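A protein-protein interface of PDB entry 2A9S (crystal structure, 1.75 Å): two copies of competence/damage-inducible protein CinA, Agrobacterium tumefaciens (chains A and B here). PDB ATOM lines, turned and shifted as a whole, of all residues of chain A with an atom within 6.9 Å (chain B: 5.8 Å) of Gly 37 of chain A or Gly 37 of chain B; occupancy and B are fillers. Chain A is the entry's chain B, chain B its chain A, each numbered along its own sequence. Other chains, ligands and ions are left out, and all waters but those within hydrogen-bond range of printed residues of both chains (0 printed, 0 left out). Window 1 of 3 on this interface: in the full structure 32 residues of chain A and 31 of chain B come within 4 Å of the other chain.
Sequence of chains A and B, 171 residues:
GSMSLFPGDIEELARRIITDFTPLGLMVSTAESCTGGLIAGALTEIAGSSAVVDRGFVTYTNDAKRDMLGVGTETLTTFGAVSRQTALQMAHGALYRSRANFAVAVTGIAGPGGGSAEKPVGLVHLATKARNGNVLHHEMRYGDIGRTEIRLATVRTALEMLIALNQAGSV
OE1 of Glu 32 of chain B is in hydrogen-bond range of N of Gly 37 of chain B, 3.0 Å away. O of Gly 41 of chain A lies within hydrogen-bond range of OG1 of Thr 44 of chain A (3.2 Å). O of Gly 41 of chain B sits at hydrogen-bond distance from OG1 of Thr 44 of chain B (3.2 Å). OE2 of Glu 32 of chain B lies within hydrogen-bond range of N of Ala 40 of chain B, 3.0 Å away. The side-chain carboxylate (OE1) of Glu 32 of chain A sits at hydrogen-bond distance from the backbone NH (N) of Leu 38 of chain A, 3.2 Å away. The backbone carbonyl oxygen (O) of Cys 34 of chain A sits at hydrogen-bond distance from the guanidinium group (NH1) of Arg 151 of chain A.
Gly 36 of chain A touches Gly 41 of chain B, and with the chains exchanged Gly 41 of chain A touches Gly 36 of chain B. Gly 36 of chain A touches Thr 44 of chain B, and with the chains exchanged Thr 44 of chain A touches Gly 36 of chain B. Gly 37 of chain B touches its own counterpart, Gly 37 of chain A. Leu 38 of chain A touches Gly 41 of chain B, and with the chains exchanged Gly 41 of chain A touches Leu 38 of chain B. Positions printed for both chains: 32, 33, 35, 36, 37, 38, 39, 40, 41, 42, 44 and 58.
Gly 36 of chain A touches Gly 37 of chain B. Gly 36 of chain A touches Thr 44 of chain B. Gly 37 of chain A touches Gly 36 of chain B (O to O, 3.6 Å). Gly 37 of chain A touches Gly 37 of chain B (CA to O, 3.6 Å). Leu 38 of chain B touches Leu 38 of chain A (CD2 to CD2, 3.95 Å). CA of Gly 41 of chain B touches CD2 of Leu 38 of chain A (3.8 Å). Leu 38 of chain B touches Gly 41 of chain A. CA of Gly 36 of chain B touches OG1 of Thr 44 of chain A (3.5 Å). Ala 40 of chain B touches Tyr 60 of chain A. CE1 of Tyr 60 of chain A touches CG2 of Thr 44 of chain B, 3.3 Å away.
Printed residues of chain B within 4 Å of Gly 41 of chain A: Gly 36 and Leu 38. Ala 42 of chain A touches none of the printed residues of chain B. Printed residues of chain B within 4 Å of Tyr 60 of chain A: Ala 40 and Thr 44. Of the printed residues of chain B, Arg 151 of chain A touches Gly 41 (2.9 Å) and Thr 44 (3.0 Å). Thr 35 of chain B touches none of the printed residues of chain A. Gly 37 of chain B touches just these residues of chain A: Gly 36 and Gly 37. Of the printed residues of chain A, Leu 38 of chain B touches Leu 38 (3.95 Å) and Gly 41 (3.8 Å). Of the printed residues of chain A, Thr 44 of chain B touches Gly 36 (3.5 Å), Tyr 60 (3.3 Å) and Arg 151 (3.0 Å). The nearest residue of chain A that does not touch Gly 37 of chain B is Leu 38 of chain A (4.5 Å).
Of the 12 printed residues of chain B, 6 touch a printed residue of chain A. Hydrophobic or aromatic side chains of chain B that line the printed part of chain A: Leu 38 and Ala 40. Hydrophobic or aromatic side chains of chain A within 4 Å of the printed part of chain B: Leu 38, Ala 40 and Tyr 60. Among the printed residues, 16 pairs touch across the chains.
The backbone NH (N) of Gly 41 of chain B lies within hydrogen-bond range of the backbone carbonyl oxygen (O) of Gly 36 of chain A (2.9 Å). The backbone carbonyl oxygen (O) of Gly 41 of chain B lies within hydrogen-bond range of the guanidinium group (NH2) of Arg 151 of chain A. The backbone carbonyl oxygen of Gly 36 of chain A lies close to the backbone carbonyl oxygen of Ala 40 of chain B (3.5 Å). The backbone carbonyl oxygen (O) of Gly 36 of chain B is in hydrogen-bond range of the backbone NH (N) of Gly 41 of chain A, at 3.0 Å. The side-chain hydroxyl (OG1) of Thr 44 of chain B is in hydrogen-bond range of the guanidinium group (NH1) of Arg 151 of chain A, at 3.0 Å. The backbone carbonyl oxygen (O) of Gly 36 of chain B lies close to the backbone carbonyl oxygen (O) of Ala 40 of chain A (3.5 Å).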
ATOM      1  N   PHE A   6      -7.688   8.310 -18.211  1.00  0.00           N
ATOM      2  CA  PHE A   6      -7.807   6.865 -18.104  1.00  0.00           C
ATOM      3  C   PHE A   6      -7.249   6.187 -19.351  1.00  0.00           C
ATOM      4  O   PHE A   6      -7.179   6.824 -20.431  1.00  0.00           O
ATOM      5  CB  PHE A   6      -9.259   6.436 -17.859  1.00  0.00           C
ATOM      6  CG  PHE A   6      -9.803   6.894 -16.524  1.00  0.00           C
ATOM      7  CD1 PHE A   6      -9.678   6.093 -15.403  1.00  0.00           C
ATOM      8  CD2 PHE A   6     -10.420   8.144 -16.409  1.00  0.00           C
ATOM      9  CE1 PHE A   6     -10.193   6.510 -14.151  1.00  0.00           C
ATOM     10  CE2 PHE A   6     -10.925   8.583 -15.139  1.00  0.00           C
ATOM     11  CZ  PHE A   6     -10.790   7.773 -14.039  1.00  0.00           C
ATOM     12  N   THR A  30     -23.296   5.477  -9.105  1.00  0.00           N
ATOM     13  CA  THR A  30     -22.211   4.585  -8.673  1.00  0.00           C
ATOM     14  C   THR A  30     -22.084   4.624  -7.163  1.00  0.00           C
ATOM     15  O   THR A  30     -22.385   5.649  -6.537  1.00  0.00           O
ATOM     16  CB  THR A  30     -20.865   4.975  -9.291  1.00  0.00           C
ATOM     17  OG1 THR A  30     -20.420   6.204  -8.702  1.00  0.00           O
ATOM     18  CG2 THR A  30     -20.987   5.109 -10.862  1.00  0.00           C
ATOM     19  N   GLU A  32     -18.926   3.480  -4.483  1.00  0.00           N
ATOM     20  CA  GLU A  32     -17.526   3.063  -4.614  1.00  0.00           C
ATOM     21  C   GLU A  32     -16.843   2.941  -3.268  1.00  0.00           C
ATOM     22  O   GLU A  32     -16.813   3.893  -2.503  1.00  0.00           O
ATOM     23  CB  GLU A  32     -16.758   4.025  -5.517  1.00  0.00           C
ATOM     24  CG  GLU A  32     -17.556   4.378  -6.787  1.00  0.00           C
ATOM     25  CD  GLU A  32     -16.801   5.194  -7.795  1.00  0.00           C
ATOM     26  OE1 GLU A  32     -15.597   4.985  -7.916  1.00  0.00           O
ATOM     27  OE2 GLU A  32     -17.425   6.014  -8.512  1.00  0.00           O
ATOM     28  N   SER A  33     -16.256   1.774  -3.045  1.00  0.00           N
ATOM     29  CA  SER A  33     -15.473   1.459  -1.868  1.00  0.00           C
ATOM     30  C   SER A  33     -14.231   0.627  -2.254  1.00  0.00           C
ATOM     31  O   SER A  33     -14.104  -0.580  -1.949  1.00  0.00           O
ATOM     32  CB  SER A  33     -16.346   0.738  -0.834  1.00  0.00           C
ATOM     33  OG  SER A  33     -15.560   0.418   0.293  1.00  0.00           O
ATOM     34  N   CYS A  34     -13.358   1.295  -2.984  1.00  0.00           N
ATOM     35  CA  CYS A  34     -11.954   0.935  -3.232  1.00  0.00           C
ATOM     36  C   CYS A  34     -11.492   1.759  -4.403  1.00  0.00           C
ATOM     37  O   CYS A  34     -10.321   2.067  -4.475  1.00  0.00           O
ATOM     38  CB  CYS A  34     -11.706  -0.558  -3.475  1.00  0.00           C
ATOM     39  SG  CYS A  34     -12.601  -1.246  -4.847  1.00  0.00           S
ATOM     40  N   THR A  35     -12.433   2.167  -5.266  1.00  0.00           N
ATOM     41  CA  THR A  35     -12.109   2.960  -6.462  1.00  0.00           C
ATOM     42  C   THR A  35     -12.159   4.464  -6.164  1.00  0.00           C
ATOM     43  O   THR A  35     -11.732   5.279  -6.978  1.00  0.00           O
ATOM     44  CB  THR A  35     -13.022   2.641  -7.677  1.00  0.00           C
ATOM     45  OG1 THR A  35     -14.418   2.683  -7.302  1.00  0.00           O
ATOM     46  CG2 THR A  35     -12.682   1.302  -8.308  1.00  0.00           C
ATOM     47  N   GLY A  36     -12.716   4.832  -5.005  1.00  0.00           N
ATOM     48  CA  GLY A  36     -12.598   6.224  -4.531  1.00  0.00           C
ATOM     49  C   GLY A  36     -13.161   7.326  -5.406  1.00  0.00           C
ATOM     50  O   GLY A  36     -12.771   8.490  -5.281  1.00  0.00           O
ATOM     51  N   GLY A  37     -14.119   6.993  -6.255  1.00  0.00           N
ATOM     52  CA  GLY A  37     -14.710   8.006  -7.142  1.00  0.00           C
ATOM     53  C   GLY A  37     -14.291   7.884  -8.590  1.00  0.00           C
ATOM     54  O   GLY A  37     -14.874   8.563  -9.449  1.00  0.00           O
ATOM     55  N   LEU A  38     -13.317   7.002  -8.854  1.00  0.00           N
ATOM     56  CA  LEU A  38     -12.785   6.790 -10.210  1.00  0.00           C
ATOM     57  C   LEU A  38     -13.794   6.220 -11.226  1.00  0.00           C
ATOM     58  O   LEU A  38     -13.615   6.437 -12.419  1.00  0.00           O
ATOM     59  CB  LEU A  38     -11.528   5.929 -10.156  1.00  0.00           C
ATOM     60  CG  LEU A  38     -10.280   6.587  -9.518  1.00  0.00           C
ATOM     61  CD1 LEU A  38      -9.061   5.622  -9.623  1.00  0.00           C
ATOM     62  CD2 LEU A  38      -9.946   8.014 -10.080  1.00  0.00           C
ATOM     63  N   ILE A  39     -14.831   5.503 -10.779  1.00  0.00           N
ATOM     64  CA  ILE A  39     -15.823   4.973 -11.733  1.00  0.00           C
ATOM     65  C   ILE A  39     -16.666   6.145 -12.237  1.00  0.00           C
ATOM     66  O   ILE A  39     -16.833   6.307 -13.459  1.00  0.00           O
ATOM     67  CB  ILE A  39     -16.747   3.852 -11.167  1.00  0.00           C
ATOM     68  CG1 ILE A  39     -15.931   2.652 -10.645  1.00  0.00           C
ATOM     69  CG2 ILE A  39     -17.762   3.402 -12.267  1.00  0.00           C
ATOM     70  CD1 ILE A  39     -16.795   1.563  -9.942  1.00  0.00           C
ATOM     71  N   ALA A  40     -17.174   6.965 -11.298  1.00  0.00           N
ATOM     72  CA  ALA A  40     -17.843   8.217 -11.682  1.00  0.00           C
ATOM     73  C   ALA A  40     -16.886   9.111 -12.475  1.00  0.00           C
ATOM     74  O   ALA A  40     -17.300   9.737 -13.454  1.00  0.00           O
ATOM     75  CB  ALA A  40     -18.389   8.948 -10.466  1.00  0.00           C
ATOM     76  N   GLY A  41     -15.613   9.136 -12.084  1.00  0.00           N
ATOM     77  CA  GLY A  41     -14.624   9.998 -12.756  1.00  0.00           C
ATOM     78  C   GLY A  41     -14.492   9.580 -14.226  1.00  0.00           C
ATOM     79  O   GLY A  41     -14.483  10.410 -15.120  1.00  0.00           O
ATOM     80  N   ALA A  42     -14.391   8.288 -14.453  1.00  0.00           N
ATOM     81  CA  ALA A  42     -14.237   7.757 -15.817  1.00  0.00           C
ATOM     82  C   ALA A  42     -15.460   8.036 -16.689  1.00  0.00           C
ATOM     83  O   ALA A  42     -15.327   8.435 -17.855  1.00  0.00           O
ATOM     84  CB  ALA A  42     -13.972   6.258 -15.770  1.00  0.00           C
ATOM     85  N   THR A  44     -17.574  10.469 -16.314  1.00  0.00           N
ATOM     86  CA  THR A  44     -17.741  11.920 -16.519  1.00  0.00           C
ATOM     87  C   THR A  44     -16.587  12.545 -17.315  1.00  0.00           C
ATOM     88  O   THR A  44     -16.590  13.739 -17.579  1.00  0.00           O
ATOM     89  CB  THR A  44     -17.974  12.664 -15.181  1.00  0.00           C
ATOM     90  OG1 THR A  44     -16.863  12.412 -14.292  1.00  0.00           O
ATOM     91  CG2 THR A  44     -19.304  12.202 -14.557  1.00  0.00           C
ATOM     92  N   PHE A  57     -21.709   7.836  -4.855  1.00  0.00           N
ATOM     93  CA  PHE A  57     -21.551   7.705  -3.415  1.00  0.00           C
ATOM     94  C   PHE A  57     -20.183   7.094  -3.186  1.00  0.00           C
ATOM     95  O   PHE A  57     -19.919   5.956  -3.611  1.00  0.00           O
ATOM     96  CB  PHE A  57     -22.577   6.741  -2.839  1.00  0.00           C
ATOM     97  CG  PHE A  57     -24.016   7.093  -3.146  1.00  0.00           C
ATOM     98  CD1 PHE A  57     -24.795   7.691  -2.185  1.00  0.00           C
ATOM     99  CD2 PHE A  57     -24.605   6.759  -4.363  1.00  0.00           C
ATOM    100  CE1 PHE A  57     -26.149   7.973  -2.431  1.00  0.00           C
ATOM    101  CE2 PHE A  57     -25.948   7.063  -4.619  1.00  0.00           C
ATOM    102  CZ  PHE A  57     -26.712   7.661  -3.657  1.00  0.00           C
ATOM    103  N   VAL A  58     -19.301   7.838  -2.541  1.00  0.00           N
ATOM    104  CA  VAL A  58     -18.001   7.284  -2.225  1.00  0.00           C
ATOM    105  C   VAL A  58     -17.968   6.954  -0.724  1.00  0.00           C
ATOM    106  O   VAL A  58     -17.951   7.856   0.102  1.00  0.00           O
ATOM    107  CB  VAL A  58     -16.854   8.232  -2.656  1.00  0.00           C
ATOM    108  CG1 VAL A  58     -15.509   7.585  -2.364  1.00  0.00           C
ATOM    109  CG2 VAL A  58     -16.980   8.560  -4.174  1.00  0.00           C
ATOM    110  N   TYR A  60     -15.976   4.637   1.640  1.00  0.00           N
ATOM    111  CA  TYR A  60     -14.850   3.827   2.114  1.00  0.00           C
ATOM    112  C   TYR A  60     -15.157   3.243   3.470  1.00  0.00           C
ATOM    113  O   TYR A  60     -14.984   2.048   3.714  1.00  0.00           O
ATOM    114  CB  TYR A  60     -13.631   4.711   2.283  1.00  0.00           C
ATOM    115  CG  TYR A  60     -13.647   5.951   1.438  1.00  0.00           C
ATOM    116  CD1 TYR A  60     -12.787   6.073   0.358  1.00  0.00           C
ATOM    117  CD2 TYR A  60     -14.533   6.991   1.705  1.00  0.00           C
ATOM    118  CE1 TYR A  60     -12.767   7.171  -0.405  1.00  0.00           C
ATOM    119  CE2 TYR A  60     -14.540   8.106   0.931  1.00  0.00           C
ATOM    120  CZ  TYR A  60     -13.649   8.194  -0.135  1.00  0.00           C
ATOM    121  OH  TYR A  60     -13.632   9.308  -0.919  1.00  0.00           O
ATOM    122  N   ARG A 151      -7.475  -0.657  -8.777  1.00  0.00           N
ATOM    123  CA  ARG A 151      -8.511   0.365  -8.973  1.00  0.00           C
ATOM    124  C   ARG A 151      -8.960   0.501 -10.461  1.00  0.00           C
ATOM    125  O   ARG A 151     -10.159   0.517 -10.778  1.00  0.00           O
ATOM    126  CB  ARG A 151      -8.026   1.666  -8.361  1.00  0.00           C
ATOM    127  CG  ARG A 151      -8.159   1.590  -6.857  1.00  0.00           C
ATOM    128  CD  ARG A 151      -7.234   2.546  -6.119  1.00  0.00           C
ATOM    129  NE  ARG A 151      -7.247   3.938  -6.530  1.00  0.00           N
ATOM    130  CZ  ARG A 151      -8.000   4.893  -5.980  1.00  0.00           C
ATOM    131  NH1 ARG A 151      -8.888   4.572  -5.033  1.00  0.00           N
ATOM    132  NH2 ARG A 151      -7.874   6.167  -6.395  1.00  0.00           N
ATOM    133  N   VAL A 155     -12.518  -0.441 -12.185  1.00  0.00           N
ATOM    134  CA  VAL A 155     -13.235   0.520 -13.076  1.00  0.00           C
ATOM    135  C   VAL A 155     -13.652  -0.188 -14.365  1.00  0.00           C
ATOM    136  O   VAL A 155     -14.822  -0.152 -14.730  1.00  0.00           O
ATOM    137  CB  VAL A 155     -12.421   1.789 -13.386  1.00  0.00           C
ATOM    138  CG1 VAL A 155     -13.140   2.666 -14.478  1.00  0.00           C
ATOM    139  CG2 VAL A 155     -12.241   2.619 -12.073  1.00  0.00           C
ATOM    140  N   GLU B  32     -18.583  16.862  -5.149  1.00  0.00           N
ATOM    141  CA  GLU B  32     -18.025  17.136  -6.462  1.00  0.00           C
ATOM    142  C   GLU B  32     -19.101  17.210  -7.525  1.00  0.00           C
ATOM    143  O   GLU B  32     -19.913  16.301  -7.675  1.00  0.00           O
ATOM    144  CB  GLU B  32     -17.015  16.045  -6.854  1.00  0.00           C
ATOM    145  CG  GLU B  32     -15.928  15.832  -5.788  1.00  0.00           C
ATOM    146  CD  GLU B  32     -14.884  14.879  -6.223  1.00  0.00           C
ATOM    147  OE1 GLU B  32     -14.403  15.038  -7.366  1.00  0.00           O
ATOM    148  OE2 GLU B  32     -14.539  14.003  -5.394  1.00  0.00           O
ATOM    149  N   SER B  33     -19.077  18.281  -8.289  1.00  0.00           N
ATOM    150  CA  SER B  33     -19.941  18.357  -9.430  1.00  0.00           C
ATOM    151  C   SER B  33     -19.022  18.072 -10.656  1.00  0.00           C
ATOM    152  O   SER B  33     -18.881  16.883 -11.099  1.00  0.00           O
ATOM    153  CB  SER B  33     -20.664  19.713  -9.389  1.00  0.00           C
ATOM    154  OG  SER B  33     -21.721  19.821 -10.341  1.00  0.00           O
ATOM    155  N   THR B  35     -15.774  17.776 -11.287  1.00  0.00           N
ATOM    156  CA  THR B  35     -14.634  16.808 -11.258  1.00  0.00           C
ATOM    157  C   THR B  35     -15.092  15.355 -11.202  1.00  0.00           C
ATOM    158  O   THR B  35     -14.291  14.434 -11.355  1.00  0.00           O
ATOM    159  CB  THR B  35     -13.699  17.031 -10.043  1.00  0.00           C
ATOM    160  OG1 THR B  35     -14.492  17.136  -8.840  1.00  0.00           O
ATOM    161  CG2 THR B  35     -12.841  18.305 -10.229  1.00  0.00           C
ATOM    162  N   GLY B  36     -16.379  15.155 -10.963  1.00  0.00           N
ATOM    163  CA  GLY B  36     -17.023  13.826 -11.104  1.00  0.00           C
ATOM    164  C   GLY B  36     -16.478  12.684 -10.231  1.00  0.00           C
ATOM    165  O   GLY B  36     -16.694  11.504 -10.547  1.00  0.00           O
ATOM    166  N   GLY B  37     -15.790  13.022  -9.140  1.00  0.00           N
ATOM    167  CA  GLY B  37     -15.212  12.009  -8.255  1.00  0.00           C
ATOM    168  C   GLY B  37     -13.685  11.986  -8.256  1.00  0.00           C
ATOM    169  O   GLY B  37     -13.090  11.259  -7.456  1.00  0.00           O
ATOM    170  N   LEU B  38     -13.049  12.741  -9.163  1.00  0.00           N
ATOM    171  CA  LEU B  38     -11.585  12.739  -9.271  1.00  0.00           C
ATOM    172  C   LEU B  38     -10.877  13.355  -8.068  1.00  0.00           C
ATOM    173  O   LEU B  38      -9.704  13.069  -7.869  1.00  0.00           O
ATOM    174  CB  LEU B  38     -11.095  13.439 -10.539  1.00  0.00           C
ATOM    175  CG  LEU B  38     -11.569  12.806 -11.848  1.00  0.00           C
ATOM    176  CD1 LEU B  38     -11.020  13.596 -13.071  1.00  0.00           C
ATOM    177  CD2 LEU B  38     -11.146  11.322 -11.882  1.00  0.00           C
ATOM    178  N   ILE B  39     -11.573  14.189  -7.278  1.00  0.00           N
ATOM    179  CA  ILE B  39     -10.897  14.726  -6.086  1.00  0.00           C
ATOM    180  C   ILE B  39     -10.726  13.597  -5.058  1.00  0.00           C
ATOM    181  O   ILE B  39      -9.599  13.364  -4.564  1.00  0.00           O
ATOM    182  CB  ILE B  39     -11.627  15.949  -5.445  1.00  0.00           C
ATOM    183  CG1 ILE B  39     -11.747  17.117  -6.442  1.00  0.00           C
ATOM    184  CG2 ILE B  39     -10.859  16.377  -4.157  1.00  0.00           C
ATOM    185  CD1 ILE B  39     -12.509  18.279  -5.885  1.00  0.00           C
ATOM    186  N   ALA B  40     -11.839  12.916  -4.720  1.00  0.00           N
ATOM    187  CA  ALA B  40     -11.753  11.702  -3.887  1.00  0.00           C
ATOM    188  C   ALA B  40     -10.800  10.692  -4.543  1.00  0.00           C
ATOM    189  O   ALA B  40     -10.029  10.041  -3.832  1.00  0.00           O
ATOM    190  CB  ALA B  40     -13.127  11.094  -3.652  1.00  0.00           C
ATOM    191  N   GLY B  41     -10.852  10.583  -5.879  1.00  0.00           N
ATOM    192  CA  GLY B  41      -9.992   9.654  -6.630  1.00  0.00           C
ATOM    193  C   GLY B  41      -8.509   9.945  -6.362  1.00  0.00           C
ATOM    194  O   GLY B  41      -7.722   9.055  -6.026  1.00  0.00           O
ATOM    195  N   ALA B  42      -8.140  11.212  -6.489  1.00  0.00           N
ATOM    196  CA  ALA B  42      -6.772  11.637  -6.246  1.00  0.00           C
ATOM    197  C   ALA B  42      -6.320  11.372  -4.806  1.00  0.00           C
ATOM    198  O   ALA B  42      -5.256  10.829  -4.597  1.00  0.00           O
ATOM    199  CB  ALA B  42      -6.564  13.092  -6.648  1.00  0.00           C
ATOM    200  N   THR B  44      -7.414   9.133  -2.783  1.00  0.00           N
ATOM    201  CA  THR B  44      -7.394   7.711  -2.451  1.00  0.00           C
ATOM    202  C   THR B  44      -6.358   6.958  -3.301  1.00  0.00           C
ATOM    203  O   THR B  44      -6.209   5.746  -3.174  1.00  0.00           O
ATOM    204  CB  THR B  44      -8.773   7.076  -2.544  1.00  0.00           C
ATOM    205  OG1 THR B  44      -9.298   7.266  -3.850  1.00  0.00           O
ATOM    206  CG2 THR B  44      -9.760   7.725  -1.547  1.00  0.00           C
ATOM    207  N   VAL B  58     -20.782  12.710  -5.193  1.00  0.00           N
ATOM    208  CA  VAL B  58     -20.656  13.221  -6.529  1.00  0.00           C
ATOM    209  C   VAL B  58     -22.054  13.628  -6.929  1.00  0.00           C
ATOM    210  O   VAL B  58     -22.905  12.780  -7.140  1.00  0.00           O
ATOM    211  CB  VAL B  58     -20.067  12.177  -7.506  1.00  0.00           C
ATOM    212  CG1 VAL B  58     -20.013  12.770  -8.918  1.00  0.00           C
ATOM    213  CG2 VAL B  58     -18.702  11.702  -7.015  1.00  0.00           C
